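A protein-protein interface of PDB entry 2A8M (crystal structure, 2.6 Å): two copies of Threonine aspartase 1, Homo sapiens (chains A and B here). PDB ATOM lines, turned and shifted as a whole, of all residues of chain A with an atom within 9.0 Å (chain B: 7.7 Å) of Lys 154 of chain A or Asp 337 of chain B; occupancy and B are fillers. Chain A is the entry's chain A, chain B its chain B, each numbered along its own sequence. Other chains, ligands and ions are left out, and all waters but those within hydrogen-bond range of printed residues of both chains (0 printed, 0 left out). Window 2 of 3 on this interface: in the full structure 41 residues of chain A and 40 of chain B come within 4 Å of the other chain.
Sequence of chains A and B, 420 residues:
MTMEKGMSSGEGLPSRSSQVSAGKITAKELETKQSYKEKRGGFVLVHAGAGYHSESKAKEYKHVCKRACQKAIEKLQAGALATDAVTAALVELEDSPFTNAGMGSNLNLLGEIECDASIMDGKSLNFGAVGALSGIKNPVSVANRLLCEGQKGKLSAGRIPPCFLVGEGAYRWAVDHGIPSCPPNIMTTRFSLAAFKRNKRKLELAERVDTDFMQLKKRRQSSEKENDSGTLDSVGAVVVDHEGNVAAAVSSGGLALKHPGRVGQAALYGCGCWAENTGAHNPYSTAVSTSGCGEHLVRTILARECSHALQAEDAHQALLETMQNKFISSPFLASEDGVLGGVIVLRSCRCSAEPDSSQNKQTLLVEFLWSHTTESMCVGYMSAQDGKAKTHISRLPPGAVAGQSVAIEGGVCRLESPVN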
ATOM      1  N   GLU A 149     -20.350  17.917 -21.264  1.00  0.00           N
ATOM      2  CA  GLU A 149     -19.412  18.888 -20.720  1.00  0.00           C
ATOM      3  C   GLU A 149     -19.174  18.547 -19.257  1.00  0.00           C
ATOM      4  O   GLU A 149     -18.047  18.584 -18.773  1.00  0.00           O
ATOM      5  CB  GLU A 149     -19.985  20.300 -20.839  1.00  0.00           C
ATOM      6  CG  GLU A 149     -20.110  20.784 -22.266  1.00  0.00           C
ATOM      7  CD  GLU A 149     -18.760  21.074 -22.901  1.00  0.00           C
ATOM      8  OE1 GLU A 149     -17.723  20.699 -22.303  1.00  0.00           O
ATOM      9  OE2 GLU A 149     -18.739  21.677 -24.000  1.00  0.00           O
ATOM     10  N   GLY A 150     -20.254  18.199 -18.569  1.00  0.00           N
ATOM     11  CA  GLY A 150     -20.167  17.852 -17.167  1.00  0.00           C
ATOM     12  C   GLY A 150     -19.325  16.625 -16.880  1.00  0.00           C
ATOM     13  O   GLY A 150     -18.927  16.412 -15.734  1.00  0.00           O
ATOM     14  N   GLN A 151     -19.051  15.811 -17.898  1.00  0.00           N
ATOM     15  CA  GLN A 151     -18.238  14.608 -17.697  1.00  0.00           C
ATOM     16  C   GLN A 151     -16.750  14.904 -17.851  1.00  0.00           C
ATOM     17  O   GLN A 151     -15.909  14.041 -17.610  1.00  0.00           O
ATOM     18  CB  GLN A 151     -18.645  13.496 -18.675  1.00  0.00           C
ATOM     19  CG  GLN A 151     -20.009  12.892 -18.395  1.00  0.00           C
ATOM     20  CD  GLN A 151     -20.361  11.763 -19.345  1.00  0.00           C
ATOM     21  OE1 GLN A 151     -20.365  11.937 -20.563  1.00  0.00           O
ATOM     22  NE2 GLN A 151     -20.667  10.598 -18.790  1.00  0.00           N
ATOM     23  N   LYS A 152     -16.433  16.127 -18.253  1.00  0.00           N
ATOM     24  CA  LYS A 152     -15.046  16.527 -18.430  1.00  0.00           C
ATOM     25  C   LYS A 152     -14.441  16.942 -17.084  1.00  0.00           C
ATOM     26  O   LYS A 152     -13.285  17.366 -17.015  1.00  0.00           O
ATOM     27  CB  LYS A 152     -14.955  17.703 -19.396  1.00  0.00           C
ATOM     28  CG  LYS A 152     -15.503  17.464 -20.777  1.00  0.00           C
ATOM     29  CD  LYS A 152     -15.383  18.765 -21.543  1.00  0.00           C
ATOM     30  CE  LYS A 152     -15.665  18.617 -23.017  1.00  0.00           C
ATOM     31  NZ  LYS A 152     -15.342  19.905 -23.698  1.00  0.00           N
ATOM     32  N   GLY A 153     -15.231  16.828 -16.021  1.00  0.00           N
ATOM     33  CA  GLY A 153     -14.746  17.197 -14.706  1.00  0.00           C
ATOM     34  C   GLY A 153     -14.497  18.687 -14.583  1.00  0.00           C
ATOM     35  O   GLY A 153     -14.895  19.463 -15.452  1.00  0.00           O
ATOM     36  N   LYS A 154     -13.830  19.085 -13.503  1.00  0.00           N
ATOM     37  CA  LYS A 154     -13.523  20.489 -13.254  1.00  0.00           C
ATOM     38  C   LYS A 154     -12.487  21.042 -14.242  1.00  0.00           C
ATOM     39  O   LYS A 154     -11.628  21.837 -13.865  1.00  0.00           O
ATOM     40  CB  LYS A 154     -13.004  20.659 -11.829  1.00  0.00           C
ATOM     41  CG  LYS A 154     -13.927  20.153 -10.744  1.00  0.00           C
ATOM     42  CD  LYS A 154     -13.288  20.363  -9.385  1.00  0.00           C
ATOM     43  CE  LYS A 154     -14.109  19.750  -8.259  1.00  0.00           C
ATOM     44  NZ  LYS A 154     -13.403  19.851  -6.942  1.00  0.00           N
ATOM     45  N   LEU A 155     -12.572  20.621 -15.501  1.00  0.00           N
ATOM     46  CA  LEU A 155     -11.647  21.081 -16.537  1.00  0.00           C
ATOM     47  C   LEU A 155     -12.038  22.462 -17.060  1.00  0.00           C
ATOM     48  O   LEU A 155     -13.085  22.631 -17.692  1.00  0.00           O
ATOM     49  CB  LEU A 155     -11.619  20.080 -17.696  1.00  0.00           C
ATOM     50  CG  LEU A 155     -10.630  18.904 -17.669  1.00  0.00           C
ATOM     51  CD1 LEU A 155     -10.610  18.228 -16.301  1.00  0.00           C
ATOM     52  CD2 LEU A 155     -11.017  17.912 -18.770  1.00  0.00           C
ATOM     53  N   GLY A 158     -12.873  24.662 -15.341  1.00  0.00           N
ATOM     54  CA  GLY A 158     -12.019  24.791 -14.174  1.00  0.00           C
ATOM     55  C   GLY A 158     -12.833  25.060 -12.924  1.00  0.00           C
ATOM     56  O   GLY A 158     -12.422  25.818 -12.044  1.00  0.00           O
ATOM     57  N   ARG A 159     -13.992  24.417 -12.850  1.00  0.00           N
ATOM     58  CA  ARG A 159     -14.919  24.572 -11.733  1.00  0.00           C
ATOM     59  C   ARG A 159     -15.916  23.422 -11.887  1.00  0.00           C
ATOM     60  O   ARG A 159     -15.971  22.794 -12.941  1.00  0.00           O
ATOM     61  CB  ARG A 159     -15.625  25.926 -11.867  1.00  0.00           C
ATOM     62  CG  ARG A 159     -16.395  26.406 -10.657  1.00  0.00           C
ATOM     63  CD  ARG A 159     -16.823  27.864 -10.842  1.00  0.00           C
ATOM     64  NE  ARG A 159     -17.834  28.011 -11.889  1.00  0.00           N
ATOM     65  CZ  ARG A 159     -17.964  29.089 -12.659  1.00  0.00           C
ATOM     66  NH1 ARG A 159     -17.145  30.124 -12.507  1.00  0.00           N
ATOM     67  NH2 ARG A 159     -18.912  29.133 -13.589  1.00  0.00           N
ATOM     68  N   ILE A 160     -16.686  23.122 -10.850  1.00  0.00           N
ATOM     69  CA  ILE A 160     -17.668  22.042 -10.953  1.00  0.00           C
ATOM     70  C   ILE A 160     -18.723  22.435 -12.000  1.00  0.00           C
ATOM     71  O   ILE A 160     -19.395  23.451 -11.866  1.00  0.00           O
ATOM     72  CB  ILE A 160     -18.346  21.783  -9.590  1.00  0.00           C
ATOM     73  CG1 ILE A 160     -17.281  21.383  -8.563  1.00  0.00           C
ATOM     74  CG2 ILE A 160     -19.395  20.688  -9.729  1.00  0.00           C
ATOM     75  CD1 ILE A 160     -17.808  21.173  -7.160  1.00  0.00           C
ATOM     76  N   PRO A 161     -18.873  21.628 -13.062  1.00  0.00           N
ATOM     77  CA  PRO A 161     -19.824  21.861 -14.156  1.00  0.00           C
ATOM     78  C   PRO A 161     -21.288  21.989 -13.748  1.00  0.00           C
ATOM     79  O   PRO A 161     -21.711  21.422 -12.745  1.00  0.00           O
ATOM     80  CB  PRO A 161     -19.601  20.655 -15.063  1.00  0.00           C
ATOM     81  CG  PRO A 161     -18.179  20.310 -14.822  1.00  0.00           C
ATOM     82  CD  PRO A 161     -18.077  20.420 -13.331  1.00  0.00           C
ATOM     83  N   PRO A 162     -22.076  22.750 -14.528  1.00  0.00           N
ATOM     84  CA  PRO A 162     -23.508  22.968 -14.278  1.00  0.00           C
ATOM     85  C   PRO A 162     -24.312  21.784 -14.809  1.00  0.00           C
ATOM     86  O   PRO A 162     -24.139  21.389 -15.962  1.00  0.00           O
ATOM     87  CB  PRO A 162     -23.830  24.239 -15.073  1.00  0.00           C
ATOM     88  CG  PRO A 162     -22.488  24.844 -15.393  1.00  0.00           C
ATOM     89  CD  PRO A 162     -21.593  23.653 -15.584  1.00  0.00           C
ATOM     90  N   CYS B 293     -22.053  22.705  -1.441  1.00  0.00           N
ATOM     91  CA  CYS B 293     -21.889  22.485  -2.873  1.00  0.00           C
ATOM     92  C   CYS B 293     -23.183  21.942  -3.478  1.00  0.00           C
ATOM     93  O   CYS B 293     -23.463  20.734  -3.422  1.00  0.00           O
ATOM     94  CB  CYS B 293     -20.731  21.510  -3.104  1.00  0.00           C
ATOM     95  SG  CYS B 293     -20.183  21.366  -4.814  1.00  0.00           S
ATOM     96  N   HIS B 296     -23.475  18.736  -5.531  1.00  0.00           N
ATOM     97  CA  HIS B 296     -23.306  17.580  -4.661  1.00  0.00           C
ATOM     98  C   HIS B 296     -24.579  17.169  -3.933  1.00  0.00           C
ATOM     99  O   HIS B 296     -24.864  15.979  -3.797  1.00  0.00           O
ATOM    100  CB  HIS B 296     -22.202  17.862  -3.643  1.00  0.00           C
ATOM    101  CG  HIS B 296     -20.836  17.950  -4.248  1.00  0.00           C
ATOM    102  ND1 HIS B 296     -19.748  18.454  -3.564  1.00  0.00           N
ATOM    103  CD2 HIS B 296     -20.381  17.599  -5.474  1.00  0.00           C
ATOM    104  CE1 HIS B 296     -18.683  18.414  -4.346  1.00  0.00           C
ATOM    105  NE2 HIS B 296     -19.042  17.900  -5.510  1.00  0.00           N
ATOM    106  N   LEU B 333     -21.085  10.532  -6.598  1.00  0.00           N
ATOM    107  CA  LEU B 333     -20.049  11.550  -6.457  1.00  0.00           C
ATOM    108  C   LEU B 333     -18.658  10.928  -6.462  1.00  0.00           C
ATOM    109  O   LEU B 333     -17.664  11.606  -6.221  1.00  0.00           O
ATOM    110  CB  LEU B 333     -20.268  12.359  -5.173  1.00  0.00           C
ATOM    111  CG  LEU B 333     -21.625  13.064  -5.062  1.00  0.00           C
ATOM    112  CD1 LEU B 333     -21.686  13.923  -3.775  1.00  0.00           C
ATOM    113  CD2 LEU B 333     -21.845  13.913  -6.322  1.00  0.00           C
ATOM    114  N   ALA B 334     -18.600   9.636  -6.758  1.00  0.00           N
ATOM    115  CA  ALA B 334     -17.339   8.909  -6.791  1.00  0.00           C
ATOM    116  C   ALA B 334     -16.272   9.624  -7.626  1.00  0.00           C
ATOM    117  O   ALA B 334     -15.076   9.369  -7.477  1.00  0.00           O
ATOM    118  CB  ALA B 334     -17.568   7.487  -7.326  1.00  0.00           C
ATOM    119  N   SER B 335     -16.707  10.527  -8.495  1.00  0.00           N
ATOM    120  CA  SER B 335     -15.783  11.266  -9.345  1.00  0.00           C
ATOM    121  C   SER B 335     -15.359  12.580  -8.698  1.00  0.00           C
ATOM    122  O   SER B 335     -14.298  13.113  -9.004  1.00  0.00           O
ATOM    123  CB  SER B 335     -16.437  11.539 -10.698  1.00  0.00           C
ATOM    124  OG  SER B 335     -16.972  10.340 -11.233  1.00  0.00           O
ATOM    125  N   GLU B 336     -16.201  13.102  -7.814  1.00  0.00           N
ATOM    126  CA  GLU B 336     -15.919  14.351  -7.123  1.00  0.00           C
ATOM    127  C   GLU B 336     -14.896  14.096  -6.033  1.00  0.00           C
ATOM    128  O   GLU B 336     -15.117  13.283  -5.139  1.00  0.00           O
ATOM    129  CB  GLU B 336     -17.191  14.911  -6.483  1.00  0.00           C
ATOM    130  CG  GLU B 336     -18.296  15.299  -7.447  1.00  0.00           C
ATOM    131  CD  GLU B 336     -17.941  16.518  -8.264  1.00  0.00           C
ATOM    132  OE1 GLU B 336     -17.345  17.461  -7.696  1.00  0.00           O
ATOM    133  OE2 GLU B 336     -18.268  16.538  -9.473  1.00  0.00           O
ATOM    134  N   ASP B 337     -13.772  14.785  -6.111  1.00  0.00           N
ATOM    135  CA  ASP B 337     -12.730  14.640  -5.110  1.00  0.00           C
ATOM    136  C   ASP B 337     -13.027  15.643  -4.008  1.00  0.00           C
ATOM    137  O   ASP B 337     -12.569  16.784  -4.055  1.00  0.00           O
ATOM    138  CB  ASP B 337     -11.372  14.928  -5.746  1.00  0.00           C
ATOM    139  CG  ASP B 337     -11.478  15.909  -6.892  1.00  0.00           C
ATOM    140  OD1 ASP B 337     -11.891  17.065  -6.644  1.00  0.00           O
ATOM    141  OD2 ASP B 337     -11.161  15.518  -8.042  1.00  0.00           O
ATOM    142  N   GLY B 338     -13.806  15.213  -3.024  1.00  0.00           N
ATOM    143  CA  GLY B 338     -14.166  16.094  -1.928  1.00  0.00           C
ATOM    144  C   GLY B 338     -15.621  16.519  -2.013  1.00  0.00           C
ATOM    145  O   GLY B 338     -16.003  17.282  -2.906  1.00  0.00           O
ATOM    146  N   VAL B 339     -16.434  16.020  -1.085  1.00  0.00           N
ATOM    147  CA  VAL B 339     -17.858  16.334  -1.051  1.00  0.00           C
ATOM    148  C   VAL B 339     -18.150  17.304   0.080  1.00  0.00           C
ATOM    149  O   VAL B 339     -17.875  17.022   1.242  1.00  0.00           O
ATOM    150  CB  VAL B 339     -18.688  15.060  -0.872  1.00  0.00           C
ATOM    151  CG1 VAL B 339     -20.153  15.411  -0.730  1.00  0.00           C
ATOM    152  CG2 VAL B 339     -18.470  14.143  -2.066  1.00  0.00           C
ATOM    153  N   LEU B 340     -18.718  18.449  -0.278  1.00  0.00           N
ATOM    154  CA  LEU B 340     -19.016  19.503   0.682  1.00  0.00           C
ATOM    155  C   LEU B 340     -20.488  19.789   0.833  1.00  0.00           C
ATOM    156  O   LEU B 340     -21.162  20.144  -0.135  1.00  0.00           O
ATOM    157  CB  LEU B 340     -18.311  20.785   0.259  1.00  0.00           C
ATOM    158  CG  LEU B 340     -16.802  20.612   0.165  1.00  0.00           C
ATOM    159  CD1 LEU B 340     -16.219  21.649  -0.766  1.00  0.00           C
ATOM    160  CD2 LEU B 340     -16.214  20.681   1.570  1.00  0.00           C
ATOM    161  N   ALA B 402     -11.492  18.554   5.163  1.00  0.00           N
ATOM    162  CA  ALA B 402     -12.845  18.943   4.790  1.00  0.00           C
ATOM    163  C   ALA B 402     -13.162  18.228   3.489  1.00  0.00           C
ATOM    164  O   ALA B 402     -12.273  17.991   2.672  1.00  0.00           O
ATOM    165  CB  ALA B 402     -12.938  20.450   4.598  1.00  0.00           C
ATOM    166  N   GLY B 403     -14.427  17.873   3.303  1.00  0.00           N
ATOM    167  CA  GLY B 403     -14.812  17.178   2.089  1.00  0.00           C
ATOM    168  C   GLY B 403     -14.321  15.744   2.120  1.00  0.00           C
ATOM    169  O   GLY B 403     -14.317  15.052   1.101  1.00  0.00           O
ATOM    170  N   GLN B 404     -13.893  15.308   3.300  1.00  0.00           N
ATOM    171  CA  GLN B 404     -13.409  13.945   3.504  1.00  0.00           C
ATOM    172  C   GLN B 404     -13.929  13.418   4.827  1.00  0.00           C
ATOM    173  O   GLN B 404     -14.095  12.215   5.001  1.00  0.00           O
ATOM    174  CB  GLN B 404     -11.881  13.902   3.520  1.00  0.00           C
ATOM    175  CG  GLN B 404     -11.247  13.518   2.200  1.00  0.00           C
ATOM    176  CD  GLN B 404     -11.754  12.179   1.683  1.00  0.00           C
ATOM    177  OE1 GLN B 404     -11.701  11.163   2.386  1.00  0.00           O
ATOM    178  NE2 GLN B 404     -12.250  12.170   0.440  1.00  0.00           N
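Lys 152 of chain A touches none of the printed residues of chain B. Printed residues of chain B within 4 Å of Lys 154 of chain A: Asp 337 (3.2 Å). Of the printed residues of chain A, Cys 293 of chain B touches Ile 160 (3.3 Å). Printed residues of chain A within 4 Å of His 296 of chain B: Ile 160 (3.9 Å). Leu 333 of chain B touches none of the printed residues of chain A. Of the printed residues of chain A, Glu 336 of chain B touches Ile 160. Asp 337 of chain B touches one residue of chain A. No residue of chain A comes within 4 Å of Gly 338 of chain B. The nearest printed residue of chain B that does not touch Lys 154 of chain A is Glu 336 of chain B (4.004 Å).
Among the printed residues, merely in contact across the chains: Ile 160 of chain A with Cys 293 of chain B, Ile 160 of chain A with His 296 of chain B and Ile 160 of chain A with Glu 336 of chain B.
The side-chain amino group (NZ) of Lys 154 of chain A lies within salt-bridge range of the side-chain carboxylate (OD1) of Asp 337 of chain B.
No position is printed for both chains.
Printed residues of chain A that touch a printed residue of chain B: Lys 154 and Ile 160. Hydrophobic or aromatic side chains of chain A within 4 Å of the printed part of chain B: Ile 160. Among the printed residues, Asp or Glu carboxylates within 4 Å of a Lys or Arg side-chain nitrogen of the other chain: Lys 154 of chain A with Asp 337 of chain B.
The side-chain sulfur (SG) of Cys 293 of chain B sits at hydrogen-bond distance from a ring nitrogen (ND1) of His 296 of chain B (3.2 Å). A ring nitrogen (ND1) of His 296 of chain B is in hydrogen-bond range of the backbone NH of Leu 340 of chain B (3.4 Å). OE1 of Glu 336 of chain B is in hydrogen-bond range of NE2 of His 296 of chain B (2.8 Å). The backbone carbonyl oxygen (O) of Leu 340 of chain B lies within hydrogen-bond range of the backbone NH (N) of Cys 293 of chain B (3.0 Å).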
